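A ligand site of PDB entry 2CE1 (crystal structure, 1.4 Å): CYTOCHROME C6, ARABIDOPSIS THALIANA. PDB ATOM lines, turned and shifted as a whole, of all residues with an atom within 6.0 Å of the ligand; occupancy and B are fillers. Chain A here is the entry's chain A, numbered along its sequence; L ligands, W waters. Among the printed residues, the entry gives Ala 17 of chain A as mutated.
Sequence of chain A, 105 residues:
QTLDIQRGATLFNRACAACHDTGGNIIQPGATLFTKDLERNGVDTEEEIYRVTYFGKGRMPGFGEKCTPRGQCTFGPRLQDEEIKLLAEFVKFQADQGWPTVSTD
O of Ala 15 touches C18 of the ligand, 3.4 Å away. Asn 25 touches the ligand (ND2 to C29, 3.3 Å). Ile 27 touches the ligand (CG2 to C31, 3.9 Å). Ala 31 touches the ligand (C to O2, 3.2 Å). CD2 of Leu 33 touches C7 of the ligand (3.4 Å). CB of Asp 37 touches O2 of the ligand, at 3.5 Å. Leu 38 touches the ligand (N to O2, 3.8 Å). Val 43 touches the ligand. Ile 49 touches the ligand. Val 52 touches the ligand (CG1 to C9, 3.7 Å). OG1 of Thr 53 touches C17 of the ligand (3.4 Å). Lys 57 touches the ligand (O to C33, 3.3 Å). N of Gly 58 touches O3 of the ligand, at 3.9 Å. Arg 59 touches the ligand. CE2 of Phe 63 touches C3 of the ligand, at 3.8 Å. CD1 of Leu 87 touches C19 of the ligand, at 3.8 Å. Hydrophobic or aromatic side chains within 4 Å of the ligand: His 20, Ile 27, Ala 31, Leu 33, Leu 38, Val 43, Ile 49, Val 52, Met 60, Phe 63 and Leu 87. The nearest printed residue that does not touch the ligand is Val 91 (4.1 Å).
The side-chain amide oxygen of Asn 25 is in hydrogen-bond range of the backbone NH of Ile 27 (3.0 Å). The side-chain amide oxygen (OD1) of Asn 41 lies close to the backbone carbonyl oxygen (O) of Asp 37 (3.2 Å). O of Phe 63 lies within hydrogen-bond range of N of Leu 79. N of Gln 28 lies within hydrogen-bond range of OD1 of Asn 25 (2.9 Å). The side-chain hydroxyl of Thr 32 sits at hydrogen-bond distance from the backbone NH of Phe 34 (3.1 Å). OE1 of Gln 28 is in hydrogen-bond range of NH2 of Arg 59. The side-chain amide oxygen of Asn 41 sits close to the backbone carbonyl oxygen of Gly 30. The backbone carbonyl oxygen (O) of Ile 49 lies within hydrogen-bond range of the side-chain hydroxyl (OG1) of Thr 53.
Water W4 lies within hydrogen-bond range of OE1 of Gln 28 (2.6 Å), N of Arg 59 (2.9 Å) and O3 of the ligand (3.0 Å).
A carbon (C25) of the ligand is bonded to the side-chain sulfur of Cys 19 (2.0 Å). The side-chain amide oxygen of Asn 41 lies close to an oxygen (O1) of the ligand. SD of Met 60 binds FE1 of the ligand, 2.3 Å away. An oxygen (O2) of the ligand sits close to the backbone carbonyl oxygen (O) of Thr 32. C18 of the ligand is covalently linked to SG of Cys 16 (1.9 Å). An iron atom (FE1) of the ligand is bound by a ring nitrogen (NE2) of His 20 (2.0 Å). An oxygen (O4) of the ligand lies within hydrogen-bond range of the side-chain amide nitrogen (NE2) of Gln 28 (3.4 Å).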
ATOM      1  N   PHE A  12     -14.431  18.615  11.918  1.00  0.00           N
ATOM      2  CA  PHE A  12     -14.735  17.920  13.157  1.00  0.00           C
ATOM      3  C   PHE A  12     -16.028  17.120  13.035  1.00  0.00           C
ATOM      4  O   PHE A  12     -16.098  15.958  13.459  1.00  0.00           O
ATOM      5  CB  PHE A  12     -14.841  18.901  14.333  1.00  0.00           C
ATOM      6  CG  PHE A  12     -15.094  18.224  15.650  1.00  0.00           C
ATOM      7  CD1 PHE A  12     -14.042  17.799  16.435  1.00  0.00           C
ATOM      8  CD2 PHE A  12     -16.401  18.009  16.099  1.00  0.00           C
ATOM      9  CE1 PHE A  12     -14.281  17.154  17.646  1.00  0.00           C
ATOM     10  CE2 PHE A  12     -16.624  17.375  17.338  1.00  0.00           C
ATOM     11  CZ  PHE A  12     -15.561  16.947  18.087  1.00  0.00           C
ATOM     12  N   ALA A  15     -15.234  13.993  10.791  1.00  0.00           N
ATOM     13  CA  ALA A  15     -14.155  13.069  11.164  1.00  0.00           C
ATOM     14  C   ALA A  15     -14.164  12.627  12.611  1.00  0.00           C
ATOM     15  O   ALA A  15     -13.490  11.654  12.956  1.00  0.00           O
ATOM     16  CB  ALA A  15     -12.778  13.673  10.840  1.00  0.00           C
ATOM     17  N   CYS A  16     -14.900  13.346  13.459  1.00  0.00           N
ATOM     18  CA  CYS A  16     -14.775  13.167  14.914  1.00  0.00           C
ATOM     19  C   CYS A  16     -16.086  13.072  15.680  1.00  0.00           C
ATOM     20  O   CYS A  16     -16.133  12.395  16.710  1.00  0.00           O
ATOM     21  CB  CYS A  16     -13.963  14.311  15.554  1.00  0.00           C
ATOM     22  SG  CYS A  16     -12.482  14.837  14.672  1.00  0.00           S
ATOM     23  N   ALA A  17     -17.109  13.790  15.230  1.00  0.00           N
ATOM     24  CA  ALA A  17     -18.306  14.001  16.050  1.00  0.00           C
ATOM     25  C   ALA A  17     -19.059  12.745  16.414  1.00  0.00           C
ATOM     26  O   ALA A  17     -19.652  12.663  17.502  1.00  0.00           O
ATOM     27  CB  ALA A  17     -19.246  14.967  15.385  1.00  0.00           C
ATOM     28  N   CYS A  19     -18.053   9.964  17.425  1.00  0.00           N
ATOM     29  CA  CYS A  19     -17.504   9.494  18.692  1.00  0.00           C
ATOM     30  C   CYS A  19     -17.498  10.564  19.785  1.00  0.00           C
ATOM     31  O   CYS A  19     -17.705  10.240  20.968  1.00  0.00           O
ATOM     32  CB  CYS A  19     -16.105   8.927  18.513  1.00  0.00           C
ATOM     33  SG  CYS A  19     -16.159   7.453  17.466  1.00  0.00           S
ATOM     34  N   HIS A  20     -17.246  11.823  19.409  1.00  0.00           N
ATOM     35  CA  HIS A  20     -17.067  12.906  20.368  1.00  0.00           C
ATOM     36  C   HIS A  20     -18.205  13.865  20.230  1.00  0.00           C
ATOM     37  O   HIS A  20     -18.004  15.058  20.057  1.00  0.00           O
ATOM     38  CB  HIS A  20     -15.726  13.612  20.162  1.00  0.00           C
ATOM     39  CG  HIS A  20     -14.554  12.734  20.458  1.00  0.00           C
ATOM     40  ND1 HIS A  20     -14.265  12.273  21.727  1.00  0.00           N
ATOM     41  CD2 HIS A  20     -13.552  12.277  19.662  1.00  0.00           C
ATOM     42  CE1 HIS A  20     -13.158  11.544  21.686  1.00  0.00           C
ATOM     43  NE2 HIS A  20     -12.694  11.545  20.451  1.00  0.00           N
ATOM     44  N   ASN A  25     -17.765  11.635  24.578  1.00  0.00           N
ATOM     45  CA  ASN A  25     -17.106  10.428  24.145  1.00  0.00           C
ATOM     46  C   ASN A  25     -18.082   9.277  24.327  1.00  0.00           C
ATOM     47  O   ASN A  25     -18.328   8.816  25.434  1.00  0.00           O
ATOM     48  CB  ASN A  25     -15.809  10.153  24.912  1.00  0.00           C
ATOM     49  CG  ASN A  25     -14.994   9.056  24.271  1.00  0.00           C
ATOM     50  OD1 ASN A  25     -15.565   8.090  23.774  1.00  0.00           O
ATOM     51  ND2 ASN A  25     -13.664   9.209  24.275  1.00  0.00           N
ATOM     52  N   ILE A  27     -17.916   6.202  23.471  1.00  0.00           N
ATOM     53  CA  ILE A  27     -17.257   4.919  23.657  1.00  0.00           C
ATOM     54  C   ILE A  27     -16.681   4.780  25.068  1.00  0.00           C
ATOM     55  O   ILE A  27     -16.787   3.709  25.676  1.00  0.00           O
ATOM     56  CB  ILE A  27     -16.077   4.777  22.628  1.00  0.00           C
ATOM     57  CG1 ILE A  27     -16.598   4.894  21.200  1.00  0.00           C
ATOM     58  CG2 ILE A  27     -15.310   3.477  22.871  1.00  0.00           C
ATOM     59  CD1 ILE A  27     -17.680   3.908  20.850  1.00  0.00           C
ATOM     60  N   GLN A  28     -16.048   5.852  25.549  1.00  0.00           N
ATOM     61  CA  GLN A  28     -15.233   5.801  26.756  1.00  0.00           C
ATOM     62  C   GLN A  28     -15.537   6.969  27.659  1.00  0.00           C
ATOM     63  O   GLN A  28     -14.996   8.070  27.491  1.00  0.00           O
ATOM     64  CB  GLN A  28     -13.734   5.797  26.423  1.00  0.00           C
ATOM     65  CG  GLN A  28     -12.836   5.623  27.650  1.00  0.00           C
ATOM     66  CD  GLN A  28     -11.428   5.270  27.299  1.00  0.00           C
ATOM     67  OE1 GLN A  28     -11.174   4.605  26.297  1.00  0.00           O
ATOM     68  NE2 GLN A  28     -10.496   5.662  28.152  1.00  0.00           N
ATOM     69  N   GLY A  30     -15.232   9.414  30.678  1.00  0.00           N
ATOM     70  CA  GLY A  30     -14.061   9.964  31.319  1.00  0.00           C
ATOM     71  C   GLY A  30     -12.987  10.439  30.364  1.00  0.00           C
ATOM     72  O   GLY A  30     -12.033  11.079  30.795  1.00  0.00           O
ATOM     73  N   ALA A  31     -13.127  10.150  29.076  1.00  0.00           N
ATOM     74  CA  ALA A  31     -12.124  10.569  28.082  1.00  0.00           C
ATOM     75  C   ALA A  31     -12.754  11.492  27.038  1.00  0.00           C
ATOM     76  O   ALA A  31     -12.559  11.327  25.833  1.00  0.00           O
ATOM     77  CB  ALA A  31     -11.493   9.381  27.426  1.00  0.00           C
ATOM     78  N   THR A  32     -13.510  12.468  27.511  1.00  0.00           N
ATOM     79  CA  THR A  32     -14.172  13.412  26.635  1.00  0.00           C
ATOM     80  C   THR A  32     -13.219  14.518  26.223  1.00  0.00           C
ATOM     81  O   THR A  32     -12.033  14.539  26.602  1.00  0.00           O
ATOM     82  CB  THR A  32     -15.403  14.054  27.305  1.00  0.00           C
ATOM     83  OG1 THR A  32     -14.966  14.989  28.302  1.00  0.00           O
ATOM     84  CG2 THR A  32     -16.313  12.997  27.943  1.00  0.00           C
ATOM     85  N   LEU A  33     -13.752  15.452  25.445  1.00  0.00           N
ATOM     86  CA  LEU A  33     -12.995  16.617  25.008  1.00  0.00           C
ATOM     87  C   LEU A  33     -13.298  17.836  25.890  1.00  0.00           C
ATOM     88  O   LEU A  33     -12.921  18.941  25.537  1.00  0.00           O
ATOM     89  CB  LEU A  33     -13.267  16.921  23.539  1.00  0.00           C
ATOM     90  CG  LEU A  33     -13.153  15.728  22.591  1.00  0.00           C
ATOM     91  CD1 LEU A  33     -13.327  16.183  21.157  1.00  0.00           C
ATOM     92  CD2 LEU A  33     -11.847  14.949  22.737  1.00  0.00           C
ATOM     93  N   PHE A  34     -13.974  17.629  27.020  1.00  0.00           N
ATOM     94  CA  PHE A  34     -14.157  18.705  27.991  1.00  0.00           C
ATOM     95  C   PHE A  34     -12.833  18.954  28.720  1.00  0.00           C
ATOM     96  O   PHE A  34     -12.040  18.019  28.955  1.00  0.00           O
ATOM     97  CB  PHE A  34     -15.249  18.354  29.000  1.00  0.00           C
ATOM     98  CG  PHE A  34     -16.645  18.432  28.441  1.00  0.00           C
ATOM     99  CD1 PHE A  34     -17.337  19.640  28.366  1.00  0.00           C
ATOM    100  CD2 PHE A  34     -17.295  17.288  28.019  1.00  0.00           C
ATOM    101  CE1 PHE A  34     -18.617  19.698  27.853  1.00  0.00           C
ATOM    102  CE2 PHE A  34     -18.596  17.354  27.516  1.00  0.00           C
ATOM    103  CZ  PHE A  34     -19.238  18.567  27.431  1.00  0.00           C
ATOM    104  N   ASP A  37     -11.605  16.542  31.588  1.00  0.00           N
ATOM    105  CA  ASP A  37     -11.047  15.242  31.202  1.00  0.00           C
ATOM    106  C   ASP A  37      -9.724  15.412  30.470  1.00  0.00           C
ATOM    107  O   ASP A  37      -8.775  14.644  30.699  1.00  0.00           O
ATOM    108  CB  ASP A  37     -12.014  14.460  30.303  1.00  0.00           C
ATOM    109  CG  ASP A  37     -13.216  13.894  31.070  1.00  0.00           C
ATOM    110  OD1 ASP A  37     -13.225  13.890  32.311  1.00  0.00           O
ATOM    111  OD2 ASP A  37     -14.171  13.457  30.391  1.00  0.00           O
ATOM    112  N   LEU A  38      -9.656  16.414  29.601  1.00  0.00           N
ATOM    113  CA  LEU A  38      -8.387  16.672  28.914  1.00  0.00           C
ATOM    114  C   LEU A  38      -7.266  16.912  29.936  1.00  0.00           C
ATOM    115  O   LEU A  38      -6.166  16.354  29.811  1.00  0.00           O
ATOM    116  CB  LEU A  38      -8.488  17.850  27.965  1.00  0.00           C
ATOM    117  CG  LEU A  38      -9.403  17.694  26.735  1.00  0.00           C
ATOM    118  CD1 LEU A  38      -9.590  19.030  26.042  1.00  0.00           C
ATOM    119  CD2 LEU A  38      -8.878  16.651  25.750  1.00  0.00           C
ATOM    120  N   ASN A  41      -6.237  13.761  31.916  1.00  0.00           N
ATOM    121  CA  ASN A  41      -5.507  12.839  31.044  1.00  0.00           C
ATOM    122  C   ASN A  41      -4.224  13.417  30.450  1.00  0.00           C
ATOM    123  O   ASN A  41      -3.585  12.780  29.646  1.00  0.00           O
ATOM    124  CB  ASN A  41      -6.471  12.298  29.980  1.00  0.00           C
ATOM    125  CG  ASN A  41      -7.663  11.603  30.624  1.00  0.00           C
ATOM    126  OD1 ASN A  41      -8.751  11.552  30.074  1.00  0.00           O
ATOM    127  ND2 ASN A  41      -7.464  11.094  31.839  1.00  0.00           N
ATOM    128  N   VAL A  43      -3.635  16.098  28.500  1.00  0.00           N
ATOM    129  CA  VAL A  43      -3.707  16.467  27.074  1.00  0.00           C
ATOM    130  C   VAL A  43      -4.522  17.727  26.778  1.00  0.00           C
ATOM    131  O   VAL A  43      -5.051  17.889  25.692  1.00  0.00           O
ATOM    132  CB  VAL A  43      -4.177  15.275  26.196  1.00  0.00           C
ATOM    133  CG1 VAL A  43      -3.182  14.133  26.300  1.00  0.00           C
ATOM    134  CG2 VAL A  43      -5.579  14.802  26.594  1.00  0.00           C
ATOM    135  N   GLU A  48      -0.747  18.448  22.531  1.00  0.00           N
ATOM    136  CA  GLU A  48      -1.151  17.111  22.976  1.00  0.00           C
ATOM    137  C   GLU A  48      -2.368  16.581  22.233  1.00  0.00           C
ATOM    138  O   GLU A  48      -2.434  15.395  21.886  1.00  0.00           O
ATOM    139  CB  GLU A  48      -1.401  17.086  24.474  1.00  0.00           C
ATOM    140  CG  GLU A  48      -0.132  17.231  25.323  1.00  0.00           C
ATOM    141  CD  GLU A  48       0.663  15.938  25.451  1.00  0.00           C
ATOM    142  OE1 GLU A  48       0.269  14.930  24.853  1.00  0.00           O
ATOM    143  OE2 GLU A  48       1.692  15.934  26.187  1.00  0.00           O
ATOM    144  N   ILE A  49      -3.335  17.463  21.981  1.00  0.00           N
ATOM    145  CA  ILE A  49      -4.496  17.101  21.185  1.00  0.00           C
ATOM    146  C   ILE A  49      -4.052  16.688  19.786  1.00  0.00           C
ATOM    147  O   ILE A  49      -4.513  15.678  19.256  1.00  0.00           O
ATOM    148  CB  ILE A  49      -5.515  18.257  21.123  1.00  0.00           C
ATOM    149  CG1 ILE A  49      -6.117  18.498  22.519  1.00  0.00           C
ATOM    150  CG2 ILE A  49      -6.605  17.947  20.106  1.00  0.00           C
ATOM    151  CD1 ILE A  49      -6.762  19.852  22.702  1.00  0.00           C
ATOM    152  N   VAL A  52      -2.392  13.065  20.037  1.00  0.00           N
ATOM    153  CA  VAL A  52      -3.322  11.935  20.176  1.00  0.00           C
ATOM    154  C   VAL A  52      -4.199  11.764  18.915  1.00  0.00           C
ATOM    155  O   VAL A  52      -4.503  10.630  18.540  1.00  0.00           O
ATOM    156  CB  VAL A  52      -4.129  12.023  21.467  1.00  0.00           C
ATOM    157  CG1 VAL A  52      -5.111  13.115  21.394  1.00  0.00           C
ATOM    158  CG2 VAL A  52      -4.810  10.679  21.772  1.00  0.00           C
ATOM    159  N   THR A  53      -4.549  12.854  18.242  1.00  0.00           N
ATOM    160  CA  THR A  53      -5.277  12.760  16.974  1.00  0.00           C
ATOM    161  C   THR A  53      -4.404  12.085  15.904  1.00  0.00           C
ATOM    162  O   THR A  53      -4.884  11.276  15.094  1.00  0.00           O
ATOM    163  CB  THR A  53      -5.794  14.132  16.512  1.00  0.00           C
ATOM    164  OG1 THR A  53      -6.555  14.736  17.566  1.00  0.00           O
ATOM    165  CG2 THR A  53      -6.641  14.017  15.259  1.00  0.00           C
ATOM    166  N   LYS A  57      -4.852   6.380  20.527  1.00  0.00           N
ATOM    167  CA  LYS A  57      -4.623   5.857  21.866  1.00  0.00           C
ATOM    168  C   LYS A  57      -5.757   4.937  22.312  1.00  0.00           C
ATOM    169  O   LYS A  57      -6.930   5.245  22.104  1.00  0.00           O
ATOM    170  CB  LYS A  57      -4.461   7.007  22.867  1.00  0.00           C
ATOM    171  CG  LYS A  57      -4.393   6.564  24.318  1.00  0.00           C
ATOM    172  CD  LYS A  57      -4.421   7.758  25.266  1.00  0.00           C
ATOM    173  CE  LYS A  57      -4.313   7.317  26.711  1.00  0.00           C
ATOM    174  NZ  LYS A  57      -3.190   6.365  26.916  1.00  0.00           N
ATOM    175  N   GLY A  58      -5.396   3.815  22.921  1.00  0.00           N
ATOM    176  CA  GLY A  58      -6.284   2.671  23.004  1.00  0.00           C
ATOM    177  C   GLY A  58      -7.284   2.638  21.860  1.00  0.00           C
ATOM    178  O   GLY A  58      -6.926   2.314  20.725  1.00  0.00           O
ATOM    179  N   ARG A  59      -8.534   2.960  22.164  1.00  0.00           N
ATOM    180  CA  ARG A  59      -9.653   2.597  21.292  1.00  0.00           C
ATOM    181  C   ARG A  59      -9.954   3.705  20.293  1.00  0.00           C
ATOM    182  O   ARG A  59     -10.868   3.586  19.468  1.00  0.00           O
ATOM    183  CB  ARG A  59     -10.899   2.296  22.122  1.00  0.00           C
ATOM    184  CG  ARG A  59     -11.198   0.813  22.277  1.00  0.00           C
ATOM    185  CD  ARG A  59     -12.393   0.505  23.164  1.00  0.00           C
ATOM    186  NE  ARG A  59     -12.422   1.347  24.360  1.00  0.00           N
ATOM    187  CZ  ARG A  59     -13.415   1.376  25.223  1.00  0.00           C
ATOM    188  NH1 ARG A  59     -14.493   0.622  25.035  1.00  0.00           N
ATOM    189  NH2 ARG A  59     -13.352   2.169  26.285  1.00  0.00           N
ATOM    190  N   MET A  60      -9.186   4.784  20.361  1.00  0.00           N
ATOM    191  CA  MET A  60      -9.206   5.801  19.350  1.00  0.00           C
ATOM    192  C   MET A  60      -8.167   5.602  18.267  1.00  0.00           C
ATOM    193  O   MET A  60      -6.965   5.596  18.566  1.00  0.00           O
ATOM    194  CB  MET A  60      -8.968   7.147  19.884  1.00  0.00           C
ATOM    195  CG  MET A  60      -9.099   8.096  18.691  1.00  0.00           C
ATOM    196  SD  MET A  60      -8.999   9.728  19.204  1.00  0.00           S
ATOM    197  CE  MET A  60      -8.168  10.638  17.907  1.00  0.00           C
ATOM    198  N   PRO A  61      -8.606   5.569  17.008  1.00  0.00           N
ATOM    199  CA  PRO A  61      -7.639   5.475  15.927  1.00  0.00           C
ATOM    200  C   PRO A  61      -6.817   6.754  15.743  1.00  0.00           C
ATOM    201  O   PRO A  61      -7.307   7.866  15.966  1.00  0.00           O
ATOM    202  CB  PRO A  61      -8.516   5.235  14.674  1.00  0.00           C
ATOM    203  CG  PRO A  61      -9.902   5.286  15.107  1.00  0.00           C
ATOM    204  CD  PRO A  61     -10.002   5.636  16.516  1.00  0.00           C
ATOM    205  N   PHE A  63      -5.004   9.346  13.035  1.00  0.00           N
ATOM    206  CA  PHE A  63      -5.357   9.876  11.718  1.00  0.00           C
ATOM    207  C   PHE A  63      -4.154  10.394  10.911  1.00  0.00           C
ATOM    208  O   PHE A  63      -4.322  10.742   9.759  1.00  0.00           O
ATOM    209  CB  PHE A  63      -6.426  10.970  11.868  1.00  0.00           C
ATOM    210  CG  PHE A  63      -7.744  10.435  12.307  1.00  0.00           C
ATOM    211  CD1 PHE A  63      -8.701  10.083  11.373  1.00  0.00           C
ATOM    212  CD2 PHE A  63      -8.011  10.226  13.651  1.00  0.00           C
ATOM    213  CE1 PHE A  63      -9.916   9.557  11.770  1.00  0.00           C
ATOM    214  CE2 PHE A  63      -9.222   9.692  14.052  1.00  0.00           C
ATOM    215  CZ  PHE A  63     -10.187   9.356  13.108  1.00  0.00           C
ATOM    216  N   LEU A  79      -5.624  11.967   7.533  1.00  0.00           N
ATOM    217  CA  LEU A  79      -5.770  13.412   7.443  1.00  0.00           C
ATOM    218  C   LEU A  79      -4.398  14.048   7.243  1.00  0.00           C
ATOM    219  O   LEU A  79      -3.395  13.536   7.744  1.00  0.00           O
ATOM    220  CB  LEU A  79      -6.412  13.972   8.714  1.00  0.00           C
ATOM    221  CG  LEU A  79      -7.882  13.575   8.953  1.00  0.00           C
ATOM    222  CD1 LEU A  79      -8.292  13.934  10.382  1.00  0.00           C
ATOM    223  CD2 LEU A  79      -8.787  14.252   7.955  1.00  0.00           C
ATOM    224  N   LEU A  87      -7.995  20.810  13.437  1.00  0.00           N
ATOM    225  CA  LEU A  87      -8.806  20.068  14.410  1.00  0.00           C
ATOM    226  C   LEU A  87      -8.328  20.275  15.852  1.00  0.00           C
ATOM    227  O   LEU A  87      -9.139  20.476  16.763  1.00  0.00           O
ATOM    228  CB  LEU A  87      -8.827  18.582  14.045  1.00  0.00           C
ATOM    229  CG  LEU A  87      -9.730  18.268  12.854  1.00  0.00           C
ATOM    230  CD1 LEU A  87      -9.439  16.902  12.305  1.00  0.00           C
ATOM    231  CD2 LEU A  87     -11.199  18.381  13.246  1.00  0.00           C
ATOM    232  N   ALA A  88      -7.013  20.256  16.085  1.00  0.00           N
ATOM    233  CA  ALA A  88      -6.485  20.423  17.439  1.00  0.00           C
ATOM    234  C   ALA A  88      -6.776  21.821  17.981  1.00  0.00           C
ATOM    235  O   ALA A  88      -7.124  22.000  19.159  1.00  0.00           O
ATOM    236  CB  ALA A  88      -4.997  20.125  17.484  1.00  0.00           C
ATOM    237  N   VAL A  91     -10.611  21.897  18.730  1.00  0.00           N
ATOM    238  CA  VAL A  91     -10.923  21.205  19.980  1.00  0.00           C
ATOM    239  C   VAL A  91     -10.493  22.036  21.187  1.00  0.00           C
ATOM    240  O   VAL A  91     -11.222  22.180  22.171  1.00  0.00           O
ATOM    241  CB  VAL A  91     -10.291  19.792  20.026  1.00  0.00           C
ATOM    242  CG1 VAL A  91     -10.396  19.193  21.406  1.00  0.00           C
ATOM    243  CG2 VAL A  91     -10.943  18.875  18.972  1.00  0.00           C
HETATM  244 FE1  LIG L   1     -10.981  10.672  19.845  1.00  0.00          FE
HETATM  245  C1  LIG L   1      -9.719  10.316  23.001  1.00  0.00           C
HETATM  246  C2  LIG L   1      -9.649  13.800  19.652  1.00  0.00           C
HETATM  247  C3  LIG L   1     -11.879  10.849  16.545  1.00  0.00           C
HETATM  248  C4  LIG L   1     -12.695   7.774  20.128  1.00  0.00           C
HETATM  249  N1  LIG L   1      -9.885  11.818  21.080  1.00  0.00           N
HETATM  250  C5  LIG L   1      -9.516  11.516  22.369  1.00  0.00           C
HETATM  251  C6  LIG L   1      -8.820  12.657  22.943  1.00  0.00           C
HETATM  252  C7  LIG L   1      -8.791  13.617  22.009  1.00  0.00           C
HETATM  253  C8  LIG L   1      -9.445  13.105  20.818  1.00  0.00           C
HETATM  254  C9  LIG L   1      -8.163  15.005  22.184  1.00  0.00           C
HETATM  255  C10 LIG L   1      -8.305  12.698  24.390  1.00  0.00           C
HETATM  256  C11 LIG L   1      -9.518  12.928  25.319  1.00  0.00           C
HETATM  257  C12 LIG L   1      -9.225  12.784  26.791  1.00  0.00           C
HETATM  258  O1  LIG L   1      -8.151  12.264  27.158  1.00  0.00           O
HETATM  259  O2  LIG L   1     -10.069  13.192  27.635  1.00  0.00           O
HETATM  260  N2  LIG L   1     -10.821  12.086  18.394  1.00  0.00           N
HETATM  261  C13 LIG L   1     -10.243  13.316  18.508  1.00  0.00           C
HETATM  262  C14 LIG L   1     -10.348  13.995  17.257  1.00  0.00           C
HETATM  263  C15 LIG L   1     -10.948  13.158  16.384  1.00  0.00           C
HETATM  264  C16 LIG L   1     -11.253  11.945  17.095  1.00  0.00           C
HETATM  265  C17 LIG L   1      -9.825  15.427  17.012  1.00  0.00           C
HETATM  266  C18 LIG L   1     -11.260  13.361  14.901  1.00  0.00           C
HETATM  267  C19 LIG L   1     -10.167  13.624  14.102  1.00  0.00           C
HETATM  268  N3  LIG L   1     -12.076   9.540  18.589  1.00  0.00           N
HETATM  269  C20 LIG L   1     -12.310   9.781  17.262  1.00  0.00           C
HETATM  270  C21 LIG L   1     -13.171   8.744  16.738  1.00  0.00           C
HETATM  271  C22 LIG L   1     -13.436   7.891  17.739  1.00  0.00           C
HETATM  272  C23 LIG L   1     -12.728   8.376  18.905  1.00  0.00           C
HETATM  273  C24 LIG L   1     -13.669   8.690  15.297  1.00  0.00           C
HETATM  274  C25 LIG L   1     -14.328   6.616  17.727  1.00  0.00           C
HETATM  275  C26 LIG L   1     -14.133   5.652  16.791  1.00  0.00           C
HETATM  276  N4  LIG L   1     -11.161   9.281  21.284  1.00  0.00           N
HETATM  277  C27 LIG L   1     -11.908   8.132  21.186  1.00  0.00           C
HETATM  278  C28 LIG L   1     -11.672   7.311  22.345  1.00  0.00           C
HETATM  279  C29 LIG L   1     -10.748   8.074  23.225  1.00  0.00           C
HETATM  280  C30 LIG L   1     -10.490   9.301  22.511  1.00  0.00           C
HETATM  281  C31 LIG L   1     -12.243   5.922  22.616  1.00  0.00           C
HETATM  282  C32 LIG L   1     -10.181   7.617  24.565  1.00  0.00           C
HETATM  283  C33 LIG L   1      -8.899   6.803  24.307  1.00  0.00           C
HETATM  284  C34 LIG L   1      -8.190   6.380  25.573  1.00  0.00           C
HETATM  285  O3  LIG L   1      -7.796   5.207  25.661  1.00  0.00           O
HETATM  286  O4  LIG L   1      -8.012   7.235  26.461  1.00  0.00           O
HETATM  287  O   HOH W   1      -7.749   7.839  29.331  1.00  0.00           O
HETATM  288  O   HOH W   2      -7.173   9.882  26.014  1.00  0.00           O
HETATM  289  O   HOH W   3      -6.259   4.586  27.678  1.00  0.00           O
HETATM  290  O   HOH W   4      -9.728   3.065  24.789  1.00  0.00           O
HETATM  291  O   HOH W   5     -13.349   4.235  19.749  1.00  0.00           O
